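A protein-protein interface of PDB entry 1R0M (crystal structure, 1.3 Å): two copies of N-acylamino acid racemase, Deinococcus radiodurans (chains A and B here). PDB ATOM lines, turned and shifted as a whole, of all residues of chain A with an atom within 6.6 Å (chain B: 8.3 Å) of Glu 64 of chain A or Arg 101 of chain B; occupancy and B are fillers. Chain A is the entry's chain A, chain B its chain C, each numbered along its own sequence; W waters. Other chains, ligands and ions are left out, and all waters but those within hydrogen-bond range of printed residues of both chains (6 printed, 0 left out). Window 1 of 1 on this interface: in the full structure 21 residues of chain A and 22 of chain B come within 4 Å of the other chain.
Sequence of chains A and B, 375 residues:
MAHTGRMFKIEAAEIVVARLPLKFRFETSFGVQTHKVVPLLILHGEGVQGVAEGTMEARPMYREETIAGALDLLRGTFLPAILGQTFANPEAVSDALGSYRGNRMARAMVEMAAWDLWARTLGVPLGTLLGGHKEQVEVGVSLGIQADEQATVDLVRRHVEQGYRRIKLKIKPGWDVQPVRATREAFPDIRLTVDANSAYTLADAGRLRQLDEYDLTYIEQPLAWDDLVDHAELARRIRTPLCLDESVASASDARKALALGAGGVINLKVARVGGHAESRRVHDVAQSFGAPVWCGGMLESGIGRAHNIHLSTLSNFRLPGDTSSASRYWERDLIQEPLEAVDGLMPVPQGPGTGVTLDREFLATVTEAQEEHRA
The backbone carbonyl oxygen of Glu 64 of chain A lies within hydrogen-bond range of the side-chain amide nitrogen of Asn 103 of chain B (2.9 Å).
The backbone carbonyl oxygen (O) of Tyr 62 of chain A is in hydrogen-bond range of the guanidinium group (NH1) of Arg 101 of chain B, 2.8 Å away.
OE1 of Glu 246 of chain A is in salt-bridge range of NH1 of Arg 101 of chain B (2.9 Å).
The backbone carbonyl oxygen of Met 61 of chain A sits close to the guanidinium group of Arg 101 of chain B (3.4 Å).
The backbone carbonyl oxygen of Glu 64 of chain B sits close to the side-chain amide oxygen of Asn 103 of chain A, 3.0 Å away.
The backbone NH of Arg 101 of chain B sits at hydrogen-bond distance from the backbone carbonyl oxygen of Pro 60 of chain A, at 2.8 Å.
The backbone carbonyl oxygen (O) of Arg 101 of chain B is in hydrogen-bond range of the side-chain amide nitrogen (ND2) of Asn 103 of chain B (2.9 Å).
Among the printed residues, pairs that only touch across the chains: Arg 59 of chain A with Tyr 100 of chain B, Pro 60 of chain A with Leu 73 of chain B, Pro 60 of chain A with Tyr 100 of chain B, Pro 60 of chain A with Asn 103 of chain B, Glu 64 of chain A with Arg 101 of chain B, Gly 102 of chain A with Trp 225 of chain B, Trp 225 of chain A with Arg 101 of chain B and Trp 225 of chain A with Gly 102 of chain B.
Of the printed residues of chain B, Gly 102 of chain A touches Trp 225 (3.8 Å).
Printed residues of chain B within 4 Å of Trp 225 of chain A: Arg 101 (3.4 Å) and Gly 102 (3.98 Å).
Arg 101 of chain B touches six residues of chain A.
Printed residues of chain A within 4 Å of Asn 103 of chain B: Pro 60 and Glu 64.
The nearest residue of chain A that does not touch Arg 101 of chain B is Ser 198 of chain A (4.1 Å).
The nearest printed residue of chain B that does not touch Gly 102 of chain A is Glu 64 of chain B (4.3 Å).
Along chain A the printed residues that touch a printed residue of chain B span positions 59 to 246.
Of the 17 printed residues of chain B, 7 touch a printed residue of chain A.
Printed residues of chain B that touch a printed residue of chain A: Glu 64, Leu 73, Tyr 100, Arg 101, Gly 102, Asn 103 and Trp 225.
Hydrophobic or aromatic side chains of chain B within 4 Å of the printed part of chain A: Leu 73, Tyr 100 and Trp 225.
Among the printed residues, 14 pairs touch across the chains.
Among the printed residues, Asp or Glu carboxylates within 4 Å of a Lys or Arg side-chain nitrogen of the other chain: Glu 246 of chain A with Arg 101 of chain B (2.9 Å).
Gly 102 of chain A touches Trp 225 of chain B, and with the chains exchanged Trp 225 of chain A touches Gly 102 of chain B.
Of the 14 pairs that touch across the chains among the printed residues, 4 have their exchanged pair printed and touching as well.
Water W1 lies within hydrogen-bond range of the side-chain amide nitrogen of Asn 103 of chain A and the backbone carbonyl oxygen of Glu 64 of chain B.
Water W6 lies within hydrogen-bond range of ND2 of Asn 103 of chain A (3.0 Å) and O of Glu 64 of chain B (3.0 Å).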
ATOM      1  N   ARG A  59      23.348  27.815   6.355  1.00  0.00           N
ATOM      2  CA  ARG A  59      23.580  27.434   4.965  1.00  0.00           C
ATOM      3  C   ARG A  59      24.977  26.830   4.834  1.00  0.00           C
ATOM      4  O   ARG A  59      25.867  27.133   5.626  1.00  0.00           O
ATOM      5  CB  ARG A  59      23.431  28.648   4.056  1.00  0.00           C
ATOM      6  CG  ARG A  59      22.009  29.172   4.016  1.00  0.00           C
ATOM      7  CD  ARG A  59      21.818  30.444   3.220  1.00  0.00           C
ATOM      8  NE  ARG A  59      20.405  30.815   3.145  1.00  0.00           N
ATOM      9  CZ  ARG A  59      19.734  31.483   4.092  1.00  0.00           C
ATOM     10  NH1 ARG A  59      20.339  31.901   5.196  1.00  0.00           N
ATOM     11  NH2 ARG A  59      18.445  31.754   3.927  1.00  0.00           N
ATOM     12  N   PRO A  60      25.180  25.968   3.842  1.00  0.00           N
ATOM     13  CA  PRO A  60      26.440  25.233   3.709  1.00  0.00           C
ATOM     14  C   PRO A  60      27.518  26.038   3.009  1.00  0.00           C
ATOM     15  O   PRO A  60      27.708  25.910   1.807  1.00  0.00           O
ATOM     16  CB  PRO A  60      26.032  24.005   2.887  1.00  0.00           C
ATOM     17  CG  PRO A  60      24.871  24.453   2.086  1.00  0.00           C
ATOM     18  CD  PRO A  60      24.172  25.548   2.851  1.00  0.00           C
ATOM     19  N   MET A  61      28.205  26.873   3.787  1.00  0.00           N
ATOM     20  CA  MET A  61      29.181  27.829   3.242  1.00  0.00           C
ATOM     21  C   MET A  61      30.626  27.379   3.465  1.00  0.00           C
ATOM     22  O   MET A  61      31.414  27.352   2.523  1.00  0.00           O
ATOM     23  CB  MET A  61      28.918  29.229   3.812  1.00  0.00           C
ATOM     24  CG  MET A  61      27.566  29.796   3.344  1.00  0.00           C
ATOM     25  SD  MET A  61      27.029  31.304   4.176  1.00  0.00           S
ATOM     26  CE  MET A  61      26.813  32.465   2.827  1.00  0.00           C
ATOM     27  N   TYR A  62      30.961  27.045   4.707  1.00  0.00           N
ATOM     28  CA  TYR A  62      32.281  26.516   5.046  1.00  0.00           C
ATOM     29  C   TYR A  62      32.396  25.045   4.658  1.00  0.00           C
ATOM     30  O   TYR A  62      33.405  24.592   4.143  1.00  0.00           O
ATOM     31  CB  TYR A  62      32.580  26.703   6.541  1.00  0.00           C
ATOM     32  CG  TYR A  62      33.761  25.869   6.977  1.00  0.00           C
ATOM     33  CD1 TYR A  62      35.063  26.243   6.680  1.00  0.00           C
ATOM     34  CD2 TYR A  62      33.567  24.663   7.610  1.00  0.00           C
ATOM     35  CE1 TYR A  62      36.130  25.454   7.055  1.00  0.00           C
ATOM     36  CE2 TYR A  62      34.618  23.870   7.973  1.00  0.00           C
ATOM     37  CZ  TYR A  62      35.897  24.259   7.696  1.00  0.00           C
ATOM     38  OH  TYR A  62      36.940  23.439   8.054  1.00  0.00           O
ATOM     39  N   ARG A  63      31.340  24.289   4.913  1.00  0.00           N
ATOM     40  CA  ARG A  63      31.270  22.913   4.461  1.00  0.00           C
ATOM     41  C   ARG A  63      29.798  22.545   4.274  1.00  0.00           C
ATOM     42  O   ARG A  63      28.961  23.421   4.118  1.00  0.00           O
ATOM     43  CB  ARG A  63      32.045  21.994   5.409  1.00  0.00           C
ATOM     44  CG  ARG A  63      33.054  21.069   4.704  1.00  0.00           C
ATOM     45  CD  ARG A  63      33.784  20.177   5.690  1.00  0.00           C
ATOM     46  NE  ARG A  63      34.751  19.254   5.097  1.00  0.00           N
ATOM     47  CZ  ARG A  63      34.446  18.054   4.607  1.00  0.00           C
ATOM     48  NH1 ARG A  63      35.397  17.287   4.084  1.00  0.00           N
ATOM     49  NH2 ARG A  63      33.190  17.623   4.612  1.00  0.00           N
ATOM     50  N   GLU A  64      29.498  21.256   4.249  1.00  0.00           N
ATOM     51  CA  GLU A  64      28.260  20.763   3.672  1.00  0.00           C
ATOM     52  C   GLU A  64      27.071  20.671   4.634  1.00  0.00           C
ATOM     53  O   GLU A  64      25.930  20.562   4.186  1.00  0.00           O
ATOM     54  CB  GLU A  64      28.524  19.398   3.031  1.00  0.00           C
ATOM     55  CG  GLU A  64      28.516  18.176   3.947  1.00  0.00           C
ATOM     56  CD  GLU A  64      29.710  18.003   4.891  1.00  0.00           C
ATOM     57  OE1 GLU A  64      29.742  16.950   5.558  1.00  0.00           O
ATOM     58  OE2 GLU A  64      30.586  18.883   5.010  1.00  0.00           O
ATOM     59  N   GLU A  65      27.314  20.699   5.940  1.00  0.00           N
ATOM     60  CA  GLU A  65      26.245  20.504   6.911  1.00  0.00           C
ATOM     61  C   GLU A  65      25.506  21.800   7.177  1.00  0.00           C
ATOM     62  O   GLU A  65      26.050  22.890   6.994  1.00  0.00           O
ATOM     63  CB  GLU A  65      26.783  19.952   8.225  1.00  0.00           C
ATOM     64  CG  GLU A  65      27.286  18.520   8.104  1.00  0.00           C
ATOM     65  CD  GLU A  65      27.947  18.024   9.366  1.00  0.00           C
ATOM     66  OE1 GLU A  65      27.211  17.696  10.320  1.00  0.00           O
ATOM     67  OE2 GLU A  65      29.194  17.961   9.407  1.00  0.00           O
ATOM     68  N   THR A  66      24.266  21.679   7.634  1.00  0.00           N
ATOM     69  CA  THR A  66      23.463  22.835   8.007  1.00  0.00           C
ATOM     70  C   THR A  66      22.794  22.607   9.350  1.00  0.00           C
ATOM     71  O   THR A  66      22.617  21.478   9.794  1.00  0.00           O
ATOM     72  CB  THR A  66      22.373  23.140   6.964  1.00  0.00           C
ATOM     73  OG1 THR A  66      21.408  22.077   6.942  1.00  0.00           O
ATOM     74  CG2 THR A  66      22.947  23.249   5.554  1.00  0.00           C
ATOM     75  N   GLY A 102      28.834  10.437   6.988  1.00  0.00           N
ATOM     76  CA  GLY A 102      29.113  11.860   6.996  1.00  0.00           C
ATOM     77  C   GLY A 102      28.600  12.547   8.238  1.00  0.00           C
ATOM     78  O   GLY A 102      28.598  11.980   9.323  1.00  0.00           O
ATOM     79  N   ASN A 103      28.147  13.776   8.071  1.00  0.00           N
ATOM     80  CA  ASN A 103      27.546  14.521   9.171  1.00  0.00           C
ATOM     81  C   ASN A 103      28.435  14.566  10.400  1.00  0.00           C
ATOM     82  O   ASN A 103      27.990  14.389  11.536  1.00  0.00           O
ATOM     83  CB  ASN A 103      26.169  13.948   9.499  1.00  0.00           C
ATOM     84  CG  ASN A 103      25.220  14.071   8.327  1.00  0.00           C
ATOM     85  OD1 ASN A 103      25.126  13.166   7.463  1.00  0.00           O
ATOM     86  ND2 ASN A 103      24.539  15.183   8.253  1.00  0.00           N
ATOM     87  N   ARG A 104      29.706  14.857  10.162  1.00  0.00           N
ATOM     88  CA  ARG A 104      30.697  14.814  11.227  1.00  0.00           C
ATOM     89  C   ARG A 104      30.477  15.865  12.295  1.00  0.00           C
ATOM     90  O   ARG A 104      30.740  15.601  13.468  1.00  0.00           O
ATOM     91  CB  ARG A 104      32.105  14.938  10.660  1.00  0.00           C
ATOM     92  CG  ARG A 104      32.489  13.756   9.772  1.00  0.00           C
ATOM     93  CD  ARG A 104      33.883  13.241   9.978  1.00  0.00           C
ATOM     94  NE  ARG A 104      34.092  11.915   9.407  1.00  0.00           N
ATOM     95  CZ  ARG A 104      34.931  10.997   9.888  1.00  0.00           C
ATOM     96  NH1 ARG A 104      35.682  11.240  10.956  1.00  0.00           N
ATOM     97  NH2 ARG A 104      35.025   9.818   9.285  1.00  0.00           N
ATOM     98  N   MET A 105      30.024  17.054  11.918  1.00  0.00           N
ATOM     99  CA  MET A 105      29.814  18.094  12.913  1.00  0.00           C
ATOM    100  C   MET A 105      28.598  17.779  13.790  1.00  0.00           C
ATOM    101  O   MET A 105      28.624  18.050  14.991  1.00  0.00           O
ATOM    102  CB  MET A 105      29.677  19.452  12.261  1.00  0.00           C
ATOM    103  CG  MET A 105      30.918  19.914  11.516  1.00  0.00           C
ATOM    104  SD  MET A 105      30.675  21.542  10.794  1.00  0.00           S
ATOM    105  CE  MET A 105      32.234  21.743   9.906  1.00  0.00           C
ATOM    106  N   ASN A 197      41.926  30.477   1.017  1.00  0.00           N
ATOM    107  CA  ASN A 197      40.471  30.430   0.947  1.00  0.00           C
ATOM    108  C   ASN A 197      39.894  29.745  -0.306  1.00  0.00           C
ATOM    109  O   ASN A 197      38.871  30.154  -0.832  1.00  0.00           O
ATOM    110  CB  ASN A 197      39.981  31.881   1.064  1.00  0.00           C
ATOM    111  CG  ASN A 197      38.500  31.996   1.320  1.00  0.00           C
ATOM    112  OD1 ASN A 197      37.838  32.904   0.788  1.00  0.00           O
ATOM    113  ND2 ASN A 197      37.961  31.098   2.124  1.00  0.00           N
ATOM    114  N   SER A 198      40.556  28.694  -0.774  1.00  0.00           N
ATOM    115  CA  SER A 198      40.121  27.935  -1.952  1.00  0.00           C
ATOM    116  C   SER A 198      39.861  28.816  -3.180  1.00  0.00           C
ATOM    117  O   SER A 198      39.032  28.500  -4.020  1.00  0.00           O
ATOM    118  CB  SER A 198      38.897  27.073  -1.626  1.00  0.00           C
ATOM    119  OG  SER A 198      39.251  26.062  -0.704  1.00  0.00           O
ATOM    120  N   ALA A 224      40.642  23.546  -4.308  1.00  0.00           N
ATOM    121  CA  ALA A 224      39.273  23.222  -3.926  1.00  0.00           C
ATOM    122  C   ALA A 224      39.196  22.701  -2.504  1.00  0.00           C
ATOM    123  O   ALA A 224      40.087  22.003  -2.026  1.00  0.00           O
ATOM    124  CB  ALA A 224      38.650  22.218  -4.900  1.00  0.00           C
ATOM    125  N   TRP A 225      38.103  23.053  -1.838  1.00  0.00           N
ATOM    126  CA  TRP A 225      37.913  22.748  -0.429  1.00  0.00           C
ATOM    127  C   TRP A 225      37.974  21.255  -0.116  1.00  0.00           C
ATOM    128  O   TRP A 225      38.417  20.872   0.968  1.00  0.00           O
ATOM    129  CB  TRP A 225      36.593  23.362   0.080  1.00  0.00           C
ATOM    130  CG  TRP A 225      35.337  22.730  -0.465  1.00  0.00           C
ATOM    131  CD1 TRP A 225      34.631  23.126  -1.567  1.00  0.00           C
ATOM    132  CD2 TRP A 225      34.618  21.615   0.081  1.00  0.00           C
ATOM    133  NE1 TRP A 225      33.540  22.312  -1.743  1.00  0.00           N
ATOM    134  CE2 TRP A 225      33.504  21.379  -0.747  1.00  0.00           C
ATOM    135  CE3 TRP A 225      34.816  20.774   1.179  1.00  0.00           C
ATOM    136  CZ2 TRP A 225      32.595  20.355  -0.508  1.00  0.00           C
ATOM    137  CZ3 TRP A 225      33.901  19.769   1.414  1.00  0.00           C
ATOM    138  CH2 TRP A 225      32.810  19.569   0.578  1.00  0.00           C
ATOM    139  N   GLU A 246      39.638  22.015   4.954  1.00  0.00           N
ATOM    140  CA  GLU A 246      38.355  21.347   4.754  1.00  0.00           C
ATOM    141  C   GLU A 246      38.488  19.924   4.255  1.00  0.00           C
ATOM    142  O   GLU A 246      37.586  19.124   4.458  1.00  0.00           O
ATOM    143  CB  GLU A 246      37.464  22.141   3.788  1.00  0.00           C
ATOM    144  CG  GLU A 246      37.007  23.518   4.258  1.00  0.00           C
ATOM    145  CD  GLU A 246      37.892  24.665   3.797  1.00  0.00           C
ATOM    146  OE1 GLU A 246      37.348  25.774   3.557  1.00  0.00           O
ATOM    147  OE2 GLU A 246      39.110  24.476   3.689  1.00  0.00           O
ATOM    148  N   ARG B  63      24.281   7.953   1.626  1.00  0.00           N
ATOM    149  CA  ARG B  63      25.265   9.026   1.643  1.00  0.00           C
ATOM    150  C   ARG B  63      24.826  10.061   2.676  1.00  0.00           C
ATOM    151  O   ARG B  63      24.053   9.752   3.581  1.00  0.00           O
ATOM    152  CB  ARG B  63      25.502   9.618   0.240  1.00  0.00           C
ATOM    153  CG  ARG B  63      26.972   9.743  -0.160  1.00  0.00           C
ATOM    154  CD  ARG B  63      27.128  10.276  -1.572  1.00  0.00           C
ATOM    155  NE  ARG B  63      28.518  10.431  -2.019  1.00  0.00           N
ATOM    156  CZ  ARG B  63      29.282  11.484  -1.756  1.00  0.00           C
ATOM    157  NH1 ARG B  63      28.832  12.492  -1.035  1.00  0.00           N
ATOM    158  NH2 ARG B  63      30.516  11.530  -2.222  1.00  0.00           N
ATOM    159  N   GLU B  64      25.327  11.277   2.554  1.00  0.00           N
ATOM    160  CA  GLU B  64      25.340  12.212   3.662  1.00  0.00           C
ATOM    161  C   GLU B  64      24.132  13.140   3.758  1.00  0.00           C
ATOM    162  O   GLU B  64      23.877  13.702   4.825  1.00  0.00           O
ATOM    163  CB  GLU B  64      26.640  13.024   3.613  1.00  0.00           C
ATOM    164  CG  GLU B  64      26.668  14.266   2.718  1.00  0.00           C
ATOM    165  CD  GLU B  64      26.688  14.025   1.207  1.00  0.00           C
ATOM    166  OE1 GLU B  64      26.805  15.021   0.462  1.00  0.00           O
ATOM    167  OE2 GLU B  64      26.591  12.879   0.727  1.00  0.00           O
ATOM    168  N   GLU B  65      23.385  13.314   2.672  1.00  0.00           N
ATOM    169  CA  GLU B  65      22.273  14.248   2.702  1.00  0.00           C
ATOM    170  C   GLU B  65      21.040  13.626   3.332  1.00  0.00           C
ATOM    171  O   GLU B  65      20.886  12.404   3.350  1.00  0.00           O
ATOM    172  CB  GLU B  65      21.961  14.741   1.301  1.00  0.00           C
ATOM    173  CG  GLU B  65      23.087  15.560   0.695  1.00  0.00           C
ATOM    174  CD  GLU B  65      22.783  15.966  -0.728  1.00  0.00           C
ATOM    175  OE1 GLU B  65      21.897  16.843  -0.942  1.00  0.00           O
ATOM    176  OE2 GLU B  65      23.421  15.391  -1.634  1.00  0.00           O
ATOM    177  N   GLY B  69      17.505  18.320   5.713  1.00  0.00           N
ATOM    178  CA  GLY B  69      18.516  19.257   5.260  1.00  0.00           C
ATOM    179  C   GLY B  69      18.256  19.769   3.853  1.00  0.00           C
ATOM    180  O   GLY B  69      18.342  20.965   3.585  1.00  0.00           O
ATOM    181  N   ALA B  70      17.931  18.850   2.951  1.00  0.00           N
ATOM    182  CA  ALA B  70      17.712  19.215   1.557  1.00  0.00           C
ATOM    183  C   ALA B  70      16.521  20.134   1.366  1.00  0.00           C
ATOM    184  O   ALA B  70      16.599  21.110   0.624  1.00  0.00           O
ATOM    185  CB  ALA B  70      17.544  17.971   0.696  1.00  0.00           C
ATOM    186  N   LEU B  73      17.264  23.585   2.560  1.00  0.00           N
ATOM    187  CA  LEU B  73      18.117  24.256   1.582  1.00  0.00           C
ATOM    188  C   LEU B  73      17.299  24.733   0.373  1.00  0.00           C
ATOM    189  O   LEU B  73      17.499  25.841  -0.118  1.00  0.00           O
ATOM    190  CB  LEU B  73      19.272  23.336   1.168  1.00  0.00           C
ATOM    191  CG  LEU B  73      20.374  23.900   0.282  1.00  0.00           C
ATOM    192  CD1 LEU B  73      21.074  25.073   0.939  1.00  0.00           C
ATOM    193  CD2 LEU B  73      21.367  22.788  -0.040  1.00  0.00           C
ATOM    194  N   PHE B  78      17.746  27.833  -2.335  1.00  0.00           N
ATOM    195  CA  PHE B  78      17.748  27.624  -3.773  1.00  0.00           C
ATOM    196  C   PHE B  78      16.502  28.186  -4.460  1.00  0.00           C
ATOM    197  O   PHE B  78      16.610  28.809  -5.522  1.00  0.00           O
ATOM    198  CB  PHE B  78      17.908  26.140  -4.117  1.00  0.00           C
ATOM    199  CG  PHE B  78      19.252  25.547  -3.758  1.00  0.00           C
ATOM    200  CD1 PHE B  78      19.412  24.169  -3.762  1.00  0.00           C
ATOM    201  CD2 PHE B  78      20.358  26.335  -3.458  1.00  0.00           C
ATOM    202  CE1 PHE B  78      20.632  23.587  -3.466  1.00  0.00           C
ATOM    203  CE2 PHE B  78      21.580  25.750  -3.148  1.00  0.00           C
ATOM    204  CZ  PHE B  78      21.717  24.370  -3.157  1.00  0.00           C
ATOM    205  N   LEU B  97      22.434  29.218  -8.371  1.00  0.00           N
ATOM    206  CA  LEU B  97      22.296  28.682  -7.012  1.00  0.00           C
ATOM    207  C   LEU B  97      23.469  29.065  -6.117  1.00  0.00           C
ATOM    208  O   LEU B  97      23.396  28.909  -4.894  1.00  0.00           O
ATOM    209  CB  LEU B  97      22.142  27.158  -7.043  1.00  0.00           C
ATOM    210  CG  LEU B  97      20.916  26.668  -7.815  1.00  0.00           C
ATOM    211  CD1 LEU B  97      20.770  25.182  -7.639  1.00  0.00           C
ATOM    212  CD2 LEU B  97      19.642  27.394  -7.402  1.00  0.00           C
ATOM    213  N   GLY B  98      24.554  29.535  -6.716  1.00  0.00           N
ATOM    214  CA  GLY B  98      25.689  30.019  -5.949  1.00  0.00           C
ATOM    215  C   GLY B  98      26.700  28.960  -5.545  1.00  0.00           C
ATOM    216  O   GLY B  98      26.688  27.818  -6.004  1.00  0.00           O
ATOM    217  N   SER B  99      27.579  29.356  -4.639  1.00  0.00           N
ATOM    218  CA  SER B  99      28.782  28.602  -4.320  1.00  0.00           C
ATOM    219  C   SER B  99      28.655  27.752  -3.063  1.00  0.00           C
ATOM    220  O   SER B  99      29.655  27.358  -2.470  1.00  0.00           O
ATOM    221  CB  SER B  99      29.959  29.575  -4.171  1.00  0.00           C
ATOM    222  OG  SER B  99      30.176  30.274  -5.384  1.00  0.00           O
ATOM    223  N   TYR B 100      27.427  27.450  -2.666  1.00  0.00           N
ATOM    224  CA  TYR B 100      27.190  26.596  -1.508  1.00  0.00           C
ATOM    225  C   TYR B 100      27.845  25.247  -1.733  1.00  0.00           C
ATOM    226  O   TYR B 100      27.888  24.748  -2.854  1.00  0.00           O
ATOM    227  CB  TYR B 100      25.690  26.456  -1.255  1.00  0.00           C
ATOM    228  CG  TYR B 100      25.076  27.792  -0.963  1.00  0.00           C
ATOM    229  CD1 TYR B 100      24.373  28.489  -1.940  1.00  0.00           C
ATOM    230  CD2 TYR B 100      25.239  28.390   0.277  1.00  0.00           C
ATOM    231  CE1 TYR B 100      23.841  29.725  -1.681  1.00  0.00           C
ATOM    232  CE2 TYR B 100      24.709  29.623   0.545  1.00  0.00           C
ATOM    233  CZ  TYR B 100      24.004  30.285  -0.436  1.00  0.00           C
ATOM    234  OH  TYR B 100      23.486  31.524  -0.159  1.00  0.00           O
ATOM    235  N   ARG B 101      28.377  24.667  -0.666  1.00  0.00           N
ATOM    236  CA  ARG B 101      29.193  23.477  -0.766  1.00  0.00           C
ATOM    237  C   ARG B 101      28.405  22.182  -0.588  1.00  0.00           C
ATOM    238  O   ARG B 101      27.485  22.098   0.223  1.00  0.00           O
ATOM    239  CB  ARG B 101      30.325  23.548   0.240  1.00  0.00           C
ATOM    240  CG  ARG B 101      31.282  24.685  -0.089  1.00  0.00           C
ATOM    241  CD  ARG B 101      32.473  24.790   0.812  1.00  0.00           C
ATOM    242  NE  ARG B 101      33.409  25.759   0.271  1.00  0.00           N
ATOM    243  CZ  ARG B 101      34.517  26.162   0.872  1.00  0.00           C
ATOM    244  NH1 ARG B 101      34.845  25.730   2.076  1.00  0.00           N
ATOM    245  NH2 ARG B 101      35.298  27.012   0.242  1.00  0.00           N
ATOM    246  N   GLY B 102      28.787  21.156  -1.342  1.00  0.00           N
ATOM    247  CA  GLY B 102      28.158  19.853  -1.261  1.00  0.00           C
ATOM    248  C   GLY B 102      26.691  19.886  -1.632  1.00  0.00           C
ATOM    249  O   GLY B 102      26.275  20.611  -2.530  1.00  0.00           O
ATOM    250  N   ASN B 103      25.906  19.072  -0.948  1.00  0.00           N
ATOM    251  CA  ASN B 103      24.451  19.044  -1.129  1.00  0.00           C
ATOM    252  C   ASN B 103      24.065  18.842  -2.590  1.00  0.00           C
ATOM    253  O   ASN B 103      23.167  19.492  -3.107  1.00  0.00           O
ATOM    254  CB  ASN B 103      23.832  20.317  -0.539  1.00  0.00           C
ATOM    255  CG  ASN B 103      24.001  20.385   0.956  1.00  0.00           C
ATOM    256  OD1 ASN B 103      23.168  19.869   1.693  1.00  0.00           O
ATOM    257  ND2 ASN B 103      25.107  20.982   1.421  1.00  0.00           N
ATOM    258  N   ARG B 104      24.736  17.911  -3.242  1.00  0.00           N
ATOM    259  CA  ARG B 104      24.535  17.687  -4.669  1.00  0.00           C
ATOM    260  C   ARG B 104      23.147  17.161  -5.008  1.00  0.00           C
ATOM    261  O   ARG B 104      22.600  17.519  -6.049  1.00  0.00           O
ATOM    262  CB  ARG B 104      25.581  16.717  -5.208  1.00  0.00           C
ATOM    263  CG  ARG B 104      26.993  17.255  -5.164  1.00  0.00           C
ATOM    264  CD  ARG B 104      27.655  17.309  -6.488  1.00  0.00           C
ATOM    265  NE  ARG B 104      28.895  18.063  -6.450  1.00  0.00           N
ATOM    266  CZ  ARG B 104      29.506  18.496  -7.535  1.00  0.00           C
ATOM    267  NH1 ARG B 104      29.005  18.218  -8.734  1.00  0.00           N
ATOM    268  NH2 ARG B 104      30.627  19.200  -7.431  1.00  0.00           N
ATOM    269  N   ARG B 107      20.789  20.092  -4.899  1.00  0.00           N
ATOM    270  CA  ARG B 107      20.997  20.845  -6.128  1.00  0.00           C
ATOM    271  C   ARG B 107      20.343  20.152  -7.315  1.00  0.00           C
ATOM    272  O   ARG B 107      19.741  20.796  -8.175  1.00  0.00           O
ATOM    273  CB  ARG B 107      22.492  20.994  -6.427  1.00  0.00           C
ATOM    274  CG  ARG B 107      23.256  21.920  -5.509  1.00  0.00           C
ATOM    275  CD  ARG B 107      24.728  22.026  -5.866  1.00  0.00           C
ATOM    276  NE  ARG B 107      25.342  23.161  -5.187  1.00  0.00           N
ATOM    277  CZ  ARG B 107      25.478  24.375  -5.707  1.00  0.00           C
ATOM    278  NH1 ARG B 107      25.081  24.644  -6.944  1.00  0.00           N
ATOM    279  NH2 ARG B 107      26.045  25.326  -4.978  1.00  0.00           N
ATOM    280  N   TRP B 225      33.032   4.304   1.506  1.00  0.00           N
ATOM    281  CA  TRP B 225      32.098   4.932   0.578  1.00  0.00           C
ATOM    282  C   TRP B 225      32.679   6.193  -0.035  1.00  0.00           C
ATOM    283  O   TRP B 225      32.344   6.543  -1.167  1.00  0.00           O
ATOM    284  CB  TRP B 225      30.749   5.220   1.261  1.00  0.00           C
ATOM    285  CG  TRP B 225      30.794   6.245   2.350  1.00  0.00           C
ATOM    286  CD1 TRP B 225      30.966   6.010   3.678  1.00  0.00           C
ATOM    287  CD2 TRP B 225      30.653   7.667   2.211  1.00  0.00           C
ATOM    288  NE1 TRP B 225      30.945   7.194   4.372  1.00  0.00           N
ATOM    289  CE2 TRP B 225      30.759   8.232   3.497  1.00  0.00           C
ATOM    290  CE3 TRP B 225      30.454   8.524   1.124  1.00  0.00           C
ATOM    291  CZ2 TRP B 225      30.666   9.603   3.723  1.00  0.00           C
ATOM    292  CZ3 TRP B 225      30.362   9.881   1.355  1.00  0.00           C
ATOM    293  CH2 TRP B 225      30.463  10.410   2.638  1.00  0.00           C
HETATM  294  O   HOH W   1      22.599  16.070   6.454  1.00  0.00           O
HETATM  295  O   HOH W   2      30.888  28.649   0.129  1.00  0.00           O
HETATM  296  O   HOH W   3      24.716  17.924   3.410  1.00  0.00           O
HETATM  297  O   HOH W   4      19.510  22.898   5.182  1.00  0.00           O
HETATM  298  O   HOH W   5      37.267  28.442   1.866  1.00  0.00           O
HETATM  299  O   HOH W   6      25.095  16.312   5.582  1.00  0.00           O
